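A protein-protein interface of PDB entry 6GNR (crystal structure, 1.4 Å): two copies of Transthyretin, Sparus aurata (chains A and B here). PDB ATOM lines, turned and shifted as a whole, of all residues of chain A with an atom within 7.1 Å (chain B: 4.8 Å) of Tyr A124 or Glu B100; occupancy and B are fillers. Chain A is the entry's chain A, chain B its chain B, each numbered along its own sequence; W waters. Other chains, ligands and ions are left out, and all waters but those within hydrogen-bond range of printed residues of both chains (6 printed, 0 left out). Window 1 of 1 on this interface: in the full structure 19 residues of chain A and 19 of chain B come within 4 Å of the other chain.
Ala A99 touches none of the printed residues of chain B.
Of the printed residues of chain B, Thr A126 touches Tyr B124.
Of the printed residues of chain A, Glu B100 touches Glu A100 (3.6 Å), Val A102 (3.3 Å) and Tyr A124 (3.2 Å).
Of the printed residues of chain A, Val B102 touches His A96 (3.3 Å).
Of the printed residues of chain A, Tyr B124 touches Glu A100, Thr A125 and Thr A126.
Of the printed residues of chain A, Thr B125 touches Ser A123 (3.98 Å), Tyr A124 (3.4 Å) and Thr A125 (2.7 Å).
Of the printed residues of chain A, Thr B126 touches His A96 (3.8 Å), Ser A123 (3.0 Å) and Tyr A124 (2.9 Å).
The nearest printed residue of chain B that does not touch Tyr A124 is Tyr B124 (4.03 Å).
The nearest residue of chain A that does not touch Glu B100 is Arg A78 (5.1 Å).
The nearest printed residue of chain B that does not touch His A96 is Glu B100 (6.2 Å).
The backbone carbonyl oxygen (O) of Glu A100 lies within hydrogen-bond range of the side-chain hydroxyl (OH) of Tyr B124 (3.3 Å).
The side-chain hydroxyl of Tyr A124 lies within hydrogen-bond range of the backbone carbonyl oxygen of Glu B100.
The side-chain hydroxyl (OG) of Ser A123 lies within hydrogen-bond range of the backbone carbonyl oxygen (O) of Thr B126 (3.0 Å).
OG1 of Thr A125 lies within hydrogen-bond range of OG1 of Thr B125 (2.7 Å).
O of Tyr B124 is in hydrogen-bond range of N of Thr A126.
The backbone carbonyl oxygen (O) of Tyr A124 sits at hydrogen-bond distance from the backbone NH (N) of Thr B126 (2.9 Å).
Val B101 touches His A96.
His A96 touches Val B102 (CA to O, 3.3 Å).
Thr B126 touches His A96 (CG2 to NE2, 3.8 Å).
Glu B100 touches Glu A100.
Val A102 touches Glu B100.
Thr B125 touches Ser A123 (CG2 to OG, 3.98 Å).
Tyr A124 touches Thr B125 (O to CA, 3.4 Å).
Thr A125 touches Tyr B124 (CA to O, 3.4 Å).
Hydrophobic or aromatic side chains of chain B that line the printed part of chain A: Val B101 and Tyr B124.
Along chain B the printed residues that touch a printed residue of chain A span positions 100 to 126.
Printed residues of chain A that touch a printed residue of chain B: His A96, Glu A100, Val A102, Ser A123, Tyr A124, Thr A125 and Thr A126.
Hydrophobic or aromatic side chains of chain A that line the printed part of chain B: His A96, Val A102 and Tyr A124.
Among the printed residues, no Asp or Glu carboxylate lies within 4 Å of a Lys or Arg side-chain nitrogen of the other chain.
Water W2 lies within hydrogen-bond range of O of Glu B100 (2.5 Å), OH of Tyr A124 (2.5 Å), O of Glu A100 (2.6 Å) and OH of Tyr B124 (2.7 Å).
Water W1 lies within hydrogen-bond range of the backbone carbonyl oxygen of Val B98 (2.7 Å), the side-chain hydroxyl of Tyr B124 (2.8 Å), the backbone NH of Val A102 (2.9 Å) and the backbone carbonyl oxygen of Glu A100 (3.5 Å).
Water W5 lies within hydrogen-bond range of O of Val A98 (2.7 Å), OH of Tyr A124 (2.8 Å) and N of Val B102 (2.9 Å).
Water W3 bridges OG1 of Thr B126 (2.8 Å) and NE2 of His A96 (2.9 Å).
Water W4 lies within hydrogen-bond range of N of Glu B100 (2.8 Å) and O of Glu A100 (3.2 Å).
Water W6 lies within hydrogen-bond range of the guanidinium group (NH1) of Arg A78 and the side-chain carboxylate (OE2) of Glu B100.
The backbone NH (N) of Leu A118 sits at hydrogen-bond distance from the backbone carbonyl oxygen (O) of Thr A125 (2.8 Å).
The backbone NH (N) of Val B79 is in hydrogen-bond range of the backbone carbonyl oxygen (O) of Val B101, 2.8 Å away.
Glu A100 touches its own counterpart, Glu B100.
Glu A100 touches Tyr B124, and with the chains exchanged Tyr A124 touches Glu B100.
Val A102 touches Glu B100, but with the chains exchanged Glu A100 does not touch Val B102 (4.3 Å).
Tyr A124 touches Thr B126, and with the chains exchanged Thr A126 touches Tyr B124.
Of the 14 pairs that touch across the chains among the printed residues, 8 have their exchanged pair printed and touching as well.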
ATOM      1  N   TRP A  49     -41.931   3.255  31.393  1.00  0.00           N
ATOM      2  CA  TRP A  49     -41.998   1.988  30.682  1.00  0.00           C
ATOM      3  C   TRP A  49     -42.465   0.905  31.639  1.00  0.00           C
ATOM      4  O   TRP A  49     -41.952   0.789  32.754  1.00  0.00           O
ATOM      5  CB  TRP A  49     -40.632   1.615  30.100  1.00  0.00           C
ATOM      6  CG  TRP A  49     -40.170   2.578  29.078  1.00  0.00           C
ATOM      7  CD1 TRP A  49     -39.299   3.604  29.261  1.00  0.00           C
ATOM      8  CD2 TRP A  49     -40.577   2.629  27.705  1.00  0.00           C
ATOM      9  NE1 TRP A  49     -39.125   4.293  28.086  1.00  0.00           N
ATOM     10  CE2 TRP A  49     -39.901   3.715  27.113  1.00  0.00           C
ATOM     11  CE3 TRP A  49     -41.444   1.864  26.918  1.00  0.00           C
ATOM     12  CZ2 TRP A  49     -40.061   4.046  25.774  1.00  0.00           C
ATOM     13  CZ3 TRP A  49     -41.607   2.207  25.595  1.00  0.00           C
ATOM     14  CH2 TRP A  49     -40.921   3.279  25.039  1.00  0.00           C
ATOM     15  N   ARG A  78     -41.362  -0.781  23.308  1.00  0.00           N
ATOM     16  CA  ARG A  78     -39.915  -0.881  23.178  1.00  0.00           C
ATOM     17  C   ARG A  78     -39.518  -2.337  23.349  1.00  0.00           C
ATOM     18  O   ARG A  78     -39.907  -2.974  24.332  1.00  0.00           O
ATOM     19  CB  ARG A  78     -39.218  -0.005  24.226  1.00  0.00           C
ATOM     20  CG  ARG A  78     -37.700  -0.144  24.308  1.00  0.00           C
ATOM     21  CD  ARG A  78     -37.149   0.687  25.467  1.00  0.00           C
ATOM     22  NE  ARG A  78     -37.322   0.050  26.769  1.00  0.00           N
ATOM     23  CZ  ARG A  78     -37.103   0.676  27.924  1.00  0.00           C
ATOM     24  NH1 ARG A  78     -36.725   1.949  27.917  1.00  0.00           N
ATOM     25  NH2 ARG A  78     -37.266   0.044  29.085  1.00  0.00           N
ATOM     26  N   THR A  83     -27.753  -7.593  23.173  1.00  0.00           N
ATOM     27  CA  THR A  83     -26.773  -8.031  22.198  1.00  0.00           C
ATOM     28  C   THR A  83     -25.373  -8.096  22.798  1.00  0.00           C
ATOM     29  O   THR A  83     -24.547  -8.881  22.326  1.00  0.00           O
ATOM     30  CB  THR A  83     -26.806  -7.097  20.977  1.00  0.00           C
ATOM     31  OG1 THR A  83     -26.568  -5.742  21.394  1.00  0.00           O
ATOM     32  CG2 THR A  83     -28.179  -7.163  20.274  1.00  0.00           C
ATOM     33  N   TRP A  87     -22.594 -11.239  22.182  1.00  0.00           N
ATOM     34  CA  TRP A  87     -21.255 -11.171  21.608  1.00  0.00           C
ATOM     35  C   TRP A  87     -20.185 -11.607  22.603  1.00  0.00           C
ATOM     36  O   TRP A  87     -19.220 -12.269  22.218  1.00  0.00           O
ATOM     37  CB  TRP A  87     -20.975  -9.773  21.054  1.00  0.00           C
ATOM     38  CG  TRP A  87     -21.781  -9.532  19.822  1.00  0.00           C
ATOM     39  CD1 TRP A  87     -22.737  -8.573  19.628  1.00  0.00           C
ATOM     40  CD2 TRP A  87     -21.748 -10.306  18.623  1.00  0.00           C
ATOM     41  NE1 TRP A  87     -23.293  -8.702  18.385  1.00  0.00           N
ATOM     42  CE2 TRP A  87     -22.699  -9.759  17.742  1.00  0.00           C
ATOM     43  CE3 TRP A  87     -20.994 -11.409  18.201  1.00  0.00           C
ATOM     44  CZ2 TRP A  87     -22.911 -10.281  16.470  1.00  0.00           C
ATOM     45  CZ3 TRP A  87     -21.206 -11.924  16.959  1.00  0.00           C
ATOM     46  CH2 TRP A  87     -22.166 -11.367  16.100  1.00  0.00           C
ATOM     47  N   HIS A  96     -22.267  -2.061  21.037  1.00  0.00           N
ATOM     48  CA  HIS A  96     -23.512  -1.606  21.645  1.00  0.00           C
ATOM     49  C   HIS A  96     -23.785  -2.341  22.955  1.00  0.00           C
ATOM     50  O   HIS A  96     -23.437  -3.511  23.129  1.00  0.00           O
ATOM     51  CB  HIS A  96     -24.687  -1.855  20.688  1.00  0.00           C
ATOM     52  CG  HIS A  96     -24.533  -1.193  19.363  1.00  0.00           C
ATOM     53  ND1 HIS A  96     -23.963  -1.829  18.286  1.00  0.00           N
ATOM     54  CD2 HIS A  96     -24.863   0.052  18.949  1.00  0.00           C
ATOM     55  CE1 HIS A  96     -23.961  -1.001  17.254  1.00  0.00           C
ATOM     56  NE2 HIS A  96     -24.494   0.149  17.632  1.00  0.00           N
ATOM     57  N   VAL A  98     -27.049  -2.653  23.925  1.00  0.00           N
ATOM     58  CA  VAL A  98     -28.287  -3.318  23.571  1.00  0.00           C
ATOM     59  C   VAL A  98     -28.634  -2.855  22.173  1.00  0.00           C
ATOM     60  O   VAL A  98     -28.058  -1.902  21.657  1.00  0.00           O
ATOM     61  CB  VAL A  98     -29.455  -2.946  24.510  1.00  0.00           C
ATOM     62  CG1 VAL A  98     -29.212  -3.481  25.940  1.00  0.00           C
ATOM     63  CG2 VAL A  98     -29.677  -1.434  24.501  1.00  0.00           C
ATOM     64  N   ALA A  99     -29.588  -3.531  21.563  1.00  0.00           N
ATOM     65  CA  ALA A  99     -30.277  -3.004  20.396  1.00  0.00           C
ATOM     66  C   ALA A  99     -31.691  -2.690  20.847  1.00  0.00           C
ATOM     67  O   ALA A  99     -32.331  -3.527  21.469  1.00  0.00           O
ATOM     68  CB  ALA A  99     -30.294  -3.996  19.233  1.00  0.00           C
ATOM     69  N   GLU A 100     -32.154  -1.475  20.575  1.00  0.00           N
ATOM     70  CA  GLU A 100     -33.482  -1.031  20.974  1.00  0.00           C
ATOM     71  C   GLU A 100     -34.330  -0.847  19.727  1.00  0.00           C
ATOM     72  O   GLU A 100     -33.870  -0.252  18.748  1.00  0.00           O
ATOM     73  CB  GLU A 100     -33.431   0.314  21.704  1.00  0.00           C
ATOM     74  CG  GLU A 100     -32.576   0.363  22.927  1.00  0.00           C
ATOM     75  CD  GLU A 100     -33.293  -0.120  24.156  1.00  0.00           C
ATOM     76  OE1 GLU A 100     -34.382  -0.726  24.038  1.00  0.00           O
ATOM     77  OE2 GLU A 100     -32.759   0.108  25.256  1.00  0.00           O
ATOM     78  N   VAL A 101     -35.566  -1.346  19.771  1.00  0.00           N
ATOM     79  CA  VAL A 101     -36.538  -1.102  18.715  1.00  0.00           C
ATOM     80  C   VAL A 101     -37.789  -0.519  19.355  1.00  0.00           C
ATOM     81  O   VAL A 101     -38.433  -1.178  20.177  1.00  0.00           O
ATOM     82  CB  VAL A 101     -36.869  -2.399  17.957  1.00  0.00           C
ATOM     83  CG1 VAL A 101     -37.930  -2.125  16.894  1.00  0.00           C
ATOM     84  CG2 VAL A 101     -35.596  -2.978  17.324  1.00  0.00           C
ATOM     85  N   VAL A 102     -38.145   0.701  18.956  1.00  0.00           N
ATOM     86  CA  VAL A 102     -39.249   1.448  19.549  1.00  0.00           C
ATOM     87  C   VAL A 102     -40.234   1.832  18.453  1.00  0.00           C
ATOM     88  O   VAL A 102     -39.833   2.398  17.434  1.00  0.00           O
ATOM     89  CB  VAL A 102     -38.737   2.711  20.259  1.00  0.00           C
ATOM     90  CG1 VAL A 102     -39.887   3.381  20.986  1.00  0.00           C
ATOM     91  CG2 VAL A 102     -37.602   2.377  21.238  1.00  0.00           C
ATOM     92  N   LEU A 117     -33.743  -8.520  12.952  1.00  0.00           N
ATOM     93  CA  LEU A 117     -32.541  -7.930  13.521  1.00  0.00           C
ATOM     94  C   LEU A 117     -31.346  -8.731  13.029  1.00  0.00           C
ATOM     95  O   LEU A 117     -31.322  -9.951  13.189  1.00  0.00           O
ATOM     96  CB  LEU A 117     -32.634  -7.959  15.050  1.00  0.00           C
ATOM     97  CG  LEU A 117     -31.516  -7.347  15.868  1.00  0.00           C
ATOM     98  CD1 LEU A 117     -31.356  -5.881  15.582  1.00  0.00           C
ATOM     99  CD2 LEU A 117     -31.827  -7.545  17.345  1.00  0.00           C
ATOM    100  N   LEU A 118     -30.354  -8.048  12.470  1.00  0.00           N
ATOM    101  CA  LEU A 118     -29.135  -8.663  11.951  1.00  0.00           C
ATOM    102  C   LEU A 118     -27.941  -8.099  12.704  1.00  0.00           C
ATOM    103  O   LEU A 118     -27.706  -6.894  12.676  1.00  0.00           O
ATOM    104  CB  LEU A 118     -28.990  -8.351  10.470  1.00  0.00           C
ATOM    105  CG  LEU A 118     -27.747  -8.866   9.750  1.00  0.00           C
ATOM    106  CD1 LEU A 118     -27.679 -10.398   9.778  1.00  0.00           C
ATOM    107  CD2 LEU A 118     -27.685  -8.356   8.300  1.00  0.00           C
ATOM    108  N   LEU A 119     -27.199  -8.971  13.377  1.00  0.00           N
ATOM    109  CA  LEU A 119     -26.194  -8.568  14.357  1.00  0.00           C
ATOM    110  C   LEU A 119     -24.767  -8.813  13.884  1.00  0.00           C
ATOM    111  O   LEU A 119     -24.441  -9.899  13.406  1.00  0.00           O
ATOM    112  CB  LEU A 119     -26.372  -9.352  15.657  1.00  0.00           C
ATOM    113  CG  LEU A 119     -27.720  -9.227  16.354  1.00  0.00           C
ATOM    114  CD1 LEU A 119     -27.687 -10.005  17.650  1.00  0.00           C
ATOM    115  CD2 LEU A 119     -28.082  -7.775  16.618  1.00  0.00           C
ATOM    116  N   SER A 120     -23.911  -7.826  14.101  1.00  0.00           N
ATOM    117  CA  SER A 120     -22.464  -7.932  14.017  1.00  0.00           C
ATOM    118  C   SER A 120     -21.895  -7.290  15.277  1.00  0.00           C
ATOM    119  O   SER A 120     -22.585  -6.521  15.952  1.00  0.00           O
ATOM    120  CB  SER A 120     -21.910  -7.203  12.789  1.00  0.00           C
ATOM    121  OG  SER A 120     -22.507  -7.681  11.602  1.00  0.00           O
ATOM    122  N   PRO A 121     -20.635  -7.562  15.617  1.00  0.00           N
ATOM    123  CA  PRO A 121     -20.131  -7.008  16.881  1.00  0.00           C
ATOM    124  C   PRO A 121     -20.207  -5.494  16.975  1.00  0.00           C
ATOM    125  O   PRO A 121     -20.468  -4.964  18.064  1.00  0.00           O
ATOM    126  CB  PRO A 121     -18.699  -7.543  16.948  1.00  0.00           C
ATOM    127  CG  PRO A 121     -18.813  -8.897  16.292  1.00  0.00           C
ATOM    128  CD  PRO A 121     -19.762  -8.649  15.130  1.00  0.00           C
ATOM    129  N   PHE A 122     -19.978  -4.775  15.874  1.00  0.00           N
ATOM    130  CA  PHE A 122     -20.018  -3.319  15.906  1.00  0.00           C
ATOM    131  C   PHE A 122     -21.192  -2.726  15.140  1.00  0.00           C
ATOM    132  O   PHE A 122     -21.207  -1.512  14.919  1.00  0.00           O
ATOM    133  CB  PHE A 122     -18.687  -2.721  15.433  1.00  0.00           C
ATOM    134  CG  PHE A 122     -17.726  -2.437  16.559  1.00  0.00           C
ATOM    135  CD1 PHE A 122     -17.247  -3.462  17.345  1.00  0.00           C
ATOM    136  CD2 PHE A 122     -17.328  -1.146  16.856  1.00  0.00           C
ATOM    137  CE1 PHE A 122     -16.376  -3.196  18.373  1.00  0.00           C
ATOM    138  CE2 PHE A 122     -16.457  -0.887  17.887  1.00  0.00           C
ATOM    139  CZ  PHE A 122     -15.994  -1.902  18.639  1.00  0.00           C
ATOM    140  N   SER A 123     -22.195  -3.525  14.777  1.00  0.00           N
ATOM    141  CA  SER A 123     -23.268  -3.023  13.927  1.00  0.00           C
ATOM    142  C   SER A 123     -24.519  -3.881  14.054  1.00  0.00           C
ATOM    143  O   SER A 123     -24.442  -5.096  14.226  1.00  0.00           O
ATOM    144  CB  SER A 123     -22.804  -3.047  12.469  1.00  0.00           C
ATOM    145  OG  SER A 123     -23.775  -2.538  11.581  1.00  0.00           O
ATOM    146  N   TYR A 124     -25.682  -3.249  13.901  1.00  0.00           N
ATOM    147  CA  TYR A 124     -26.887  -4.022  13.666  1.00  0.00           C
ATOM    148  C   TYR A 124     -27.766  -3.323  12.642  1.00  0.00           C
ATOM    149  O   TYR A 124     -27.722  -2.104  12.482  1.00  0.00           O
ATOM    150  CB  TYR A 124     -27.659  -4.379  14.937  1.00  0.00           C
ATOM    151  CG  TYR A 124     -28.139  -3.201  15.761  1.00  0.00           C
ATOM    152  CD1 TYR A 124     -29.376  -2.624  15.536  1.00  0.00           C
ATOM    153  CD2 TYR A 124     -27.365  -2.688  16.792  1.00  0.00           C
ATOM    154  CE1 TYR A 124     -29.832  -1.567  16.299  1.00  0.00           C
ATOM    155  CE2 TYR A 124     -27.801  -1.647  17.554  1.00  0.00           C
ATOM    156  CZ  TYR A 124     -29.033  -1.086  17.320  1.00  0.00           C
ATOM    157  OH  TYR A 124     -29.451  -0.036  18.111  1.00  0.00           O
ATOM    158  N   THR A 125     -28.560  -4.133  11.955  1.00  0.00           N
ATOM    159  CA  THR A 125     -29.618  -3.678  11.069  1.00  0.00           C
ATOM    160  C   THR A 125     -30.931  -4.162  11.645  1.00  0.00           C
ATOM    161  O   THR A 125     -31.071  -5.339  11.991  1.00  0.00           O
ATOM    162  CB  THR A 125     -29.439  -4.265   9.669  1.00  0.00           C
ATOM    163  OG1 THR A 125     -28.220  -3.777   9.114  1.00  0.00           O
ATOM    164  CG2 THR A 125     -30.616  -3.911   8.751  1.00  0.00           C
ATOM    165  N   THR A 126     -31.903  -3.285  11.693  1.00  0.00           N
ATOM    166  CA  THR A 126     -33.210  -3.725  12.111  1.00  0.00           C
ATOM    167  C   THR A 126     -34.277  -3.193  11.178  1.00  0.00           C
ATOM    168  O   THR A 126     -34.254  -2.026  10.772  1.00  0.00           O
ATOM    169  CB  THR A 126     -33.474  -3.359  13.548  1.00  0.00           C
ATOM    170  OG1 THR A 126     -34.634  -4.059  13.968  1.00  0.00           O
ATOM    171  CG2 THR A 126     -33.658  -1.834  13.764  1.00  0.00           C
ATOM    172  N   ARG B  78     -26.234   7.136  25.302  1.00  0.00           N
ATOM    173  CA  ARG B  78     -27.298   6.901  24.342  1.00  0.00           C
ATOM    174  C   ARG B  78     -27.401   8.116  23.436  1.00  0.00           C
ATOM    175  O   ARG B  78     -27.422   9.252  23.913  1.00  0.00           O
ATOM    176  CB  ARG B  78     -28.630   6.711  25.087  1.00  0.00           C
ATOM    177  CG  ARG B  78     -29.891   6.606  24.255  1.00  0.00           C
ATOM    178  CD  ARG B  78     -31.107   6.486  25.166  1.00  0.00           C
ATOM    179  NE  ARG B  78     -31.486   7.736  25.840  1.00  0.00           N
ATOM    180  CZ  ARG B  78     -32.415   7.810  26.800  1.00  0.00           C
ATOM    181  NH1 ARG B  78     -33.027   6.708  27.222  1.00  0.00           N
ATOM    182  NH2 ARG B  78     -32.738   8.975  27.358  1.00  0.00           N
ATOM    183  N   VAL B  79     -27.481   7.878  22.136  1.00  0.00           N
ATOM    184  CA  VAL B  79     -27.834   8.921  21.190  1.00  0.00           C
ATOM    185  C   VAL B  79     -29.190   8.562  20.612  1.00  0.00           C
ATOM    186  O   VAL B  79     -29.367   7.479  20.035  1.00  0.00           O
ATOM    187  CB  VAL B  79     -26.775   9.098  20.098  1.00  0.00           C
ATOM    188  CG1 VAL B  79     -27.189  10.211  19.133  1.00  0.00           C
ATOM    189  CG2 VAL B  79     -25.408   9.377  20.718  1.00  0.00           C
ATOM    190  N   GLU B  80     -30.129   9.489  20.738  1.00  0.00           N
ATOM    191  CA  GLU B  80     -31.501   9.299  20.305  1.00  0.00           C
ATOM    192  C   GLU B  80     -31.719  10.155  19.063  1.00  0.00           C
ATOM    193  O   GLU B  80     -31.763  11.388  19.149  1.00  0.00           O
ATOM    194  CB  GLU B  80     -32.446   9.731  21.420  1.00  0.00           C
ATOM    195  CG  GLU B  80     -33.867   9.560  21.024  1.00  0.00           C
ATOM    196  CD  GLU B  80     -34.841  10.077  22.039  1.00  0.00           C
ATOM    197  OE1 GLU B  80     -35.002   9.390  23.058  1.00  0.00           O
ATOM    198  OE2 GLU B  80     -35.437  11.154  21.819  1.00  0.00           O
ATOM    199  N   VAL B  98     -38.249   6.291  17.140  1.00  0.00           N
ATOM    200  CA  VAL B  98     -36.951   6.918  17.340  1.00  0.00           C
ATOM    201  C   VAL B  98     -35.925   5.850  17.002  1.00  0.00           C
ATOM    202  O   VAL B  98     -36.254   4.666  16.946  1.00  0.00           O
ATOM    203  CB  VAL B  98     -36.859   7.372  18.820  1.00  0.00           C
ATOM    204  CG1 VAL B  98     -36.776   6.183  19.764  1.00  0.00           C
ATOM    205  CG2 VAL B  98     -35.740   8.262  19.059  1.00  0.00           C
ATOM    206  N   ALA B  99     -34.689   6.264  16.736  1.00  0.00           N
ATOM    207  CA  ALA B  99     -33.570   5.329  16.617  1.00  0.00           C
ATOM    208  C   ALA B  99     -32.608   5.632  17.751  1.00  0.00           C
ATOM    209  O   ALA B  99     -32.001   6.694  17.781  1.00  0.00           O
ATOM    210  CB  ALA B  99     -32.846   5.463  15.283  1.00  0.00           C
ATOM    211  N   GLU B 100     -32.463   4.707  18.685  1.00  0.00           N
ATOM    212  CA  GLU B 100     -31.553   4.875  19.807  1.00  0.00           C
ATOM    213  C   GLU B 100     -30.313   4.014  19.607  1.00  0.00           C
ATOM    214  O   GLU B 100     -30.420   2.830  19.290  1.00  0.00           O
ATOM    215  CB  GLU B 100     -32.235   4.479  21.111  1.00  0.00           C
ATOM    216  CG  GLU B 100     -33.284   5.442  21.568  1.00  0.00           C
ATOM    217  CD  GLU B 100     -34.215   4.791  22.538  1.00  0.00           C
ATOM    218  OE1 GLU B 100     -34.690   3.678  22.216  1.00  0.00           O
ATOM    219  OE2 GLU B 100     -34.435   5.359  23.628  1.00  0.00           O
ATOM    220  N   VAL B 101     -29.147   4.611  19.822  1.00  0.00           N
ATOM    221  CA  VAL B 101     -27.865   3.909  19.782  1.00  0.00           C
ATOM    222  C   VAL B 101     -27.255   4.016  21.172  1.00  0.00           C
ATOM    223  O   VAL B 101     -26.970   5.121  21.638  1.00  0.00           O
ATOM    224  CB  VAL B 101     -26.935   4.507  18.718  1.00  0.00           C
ATOM    225  CG1 VAL B 101     -25.580   3.811  18.728  1.00  0.00           C
ATOM    226  CG2 VAL B 101     -27.589   4.379  17.336  1.00  0.00           C
ATOM    227  N   VAL B 102     -27.063   2.870  21.826  1.00  0.00           N
ATOM    228  CA  VAL B 102     -26.630   2.804  23.218  1.00  0.00           C
ATOM    229  C   VAL B 102     -25.316   2.035  23.248  1.00  0.00           C
ATOM    230  O   VAL B 102     -25.267   0.885  22.800  1.00  0.00           O
ATOM    231  CB  VAL B 102     -27.684   2.107  24.098  1.00  0.00           C
ATOM    232  CG1 VAL B 102     -27.247   2.122  25.569  1.00  0.00           C
ATOM    233  CG2 VAL B 102     -29.068   2.729  23.934  1.00  0.00           C
ATOM    234  N   TYR B 124     -33.281   0.641   9.819  1.00  0.00           N
ATOM    235  CA  TYR B 124     -32.023   1.362   9.877  1.00  0.00           C
ATOM    236  C   TYR B 124     -30.891   0.405  10.196  1.00  0.00           C
ATOM    237  O   TYR B 124     -31.091  -0.646  10.817  1.00  0.00           O
ATOM    238  CB  TYR B 124     -32.003   2.584  10.811  1.00  0.00           C
ATOM    239  CG  TYR B 124     -32.384   2.314  12.236  1.00  0.00           C
ATOM    240  CD1 TYR B 124     -31.439   1.966  13.192  1.00  0.00           C
ATOM    241  CD2 TYR B 124     -33.701   2.442  12.630  1.00  0.00           C
ATOM    242  CE1 TYR B 124     -31.815   1.740  14.518  1.00  0.00           C
ATOM    243  CE2 TYR B 124     -34.082   2.227  13.919  1.00  0.00           C
ATOM    244  CZ  TYR B 124     -33.146   1.870  14.857  1.00  0.00           C
ATOM    245  OH  TYR B 124     -33.567   1.668  16.136  1.00  0.00           O
ATOM    246  N   THR B 125     -29.705   0.803   9.754  1.00  0.00           N
ATOM    247  CA  THR B 125     -28.457   0.127  10.067  1.00  0.00           C
ATOM    248  C   THR B 125     -27.590   1.107  10.831  1.00  0.00           C
ATOM    249  O   THR B 125     -27.416   2.254  10.399  1.00  0.00           O
ATOM    250  CB  THR B 125     -27.755  -0.307   8.785  1.00  0.00           C
ATOM    251  OG1 THR B 125     -28.553  -1.291   8.130  1.00  0.00           O
ATOM    252  CG2 THR B 125     -26.378  -0.889   9.057  1.00  0.00           C
ATOM    253  N   THR B 126     -26.982   0.633  11.891  1.00  0.00           N
ATOM    254  CA  THR B 126     -26.079   1.500  12.598  1.00  0.00           C
ATOM    255  C   THR B 126     -24.815   0.754  12.964  1.00  0.00           C
ATOM    256  O   THR B 126     -24.844  -0.413  13.370  1.00  0.00           O
ATOM    257  CB  THR B 126     -26.737   2.121  13.800  1.00  0.00           C
ATOM    258  OG1 THR B 126     -25.880   3.152  14.280  1.00  0.00           O
ATOM    259  CG2 THR B 126     -27.024   1.070  14.889  1.00  0.00           C
HETATM  260  O   HOH W   1     -36.078   1.999  17.332  1.00  0.00           O
HETATM  261  O   HOH W   2     -31.729   1.098  18.020  1.00  0.00           O
HETATM  262  O   HOH W   3     -23.874   2.518  16.084  1.00  0.00           O
HETATM  263  O   HOH W   4     -34.392   2.833  19.463  1.00  0.00           O
HETATM  264  O   HOH W   5     -27.992   0.540  20.450  1.00  0.00           O
HETATM  265  O   HOH W   6     -35.882   3.801  25.896  1.00  0.00           O
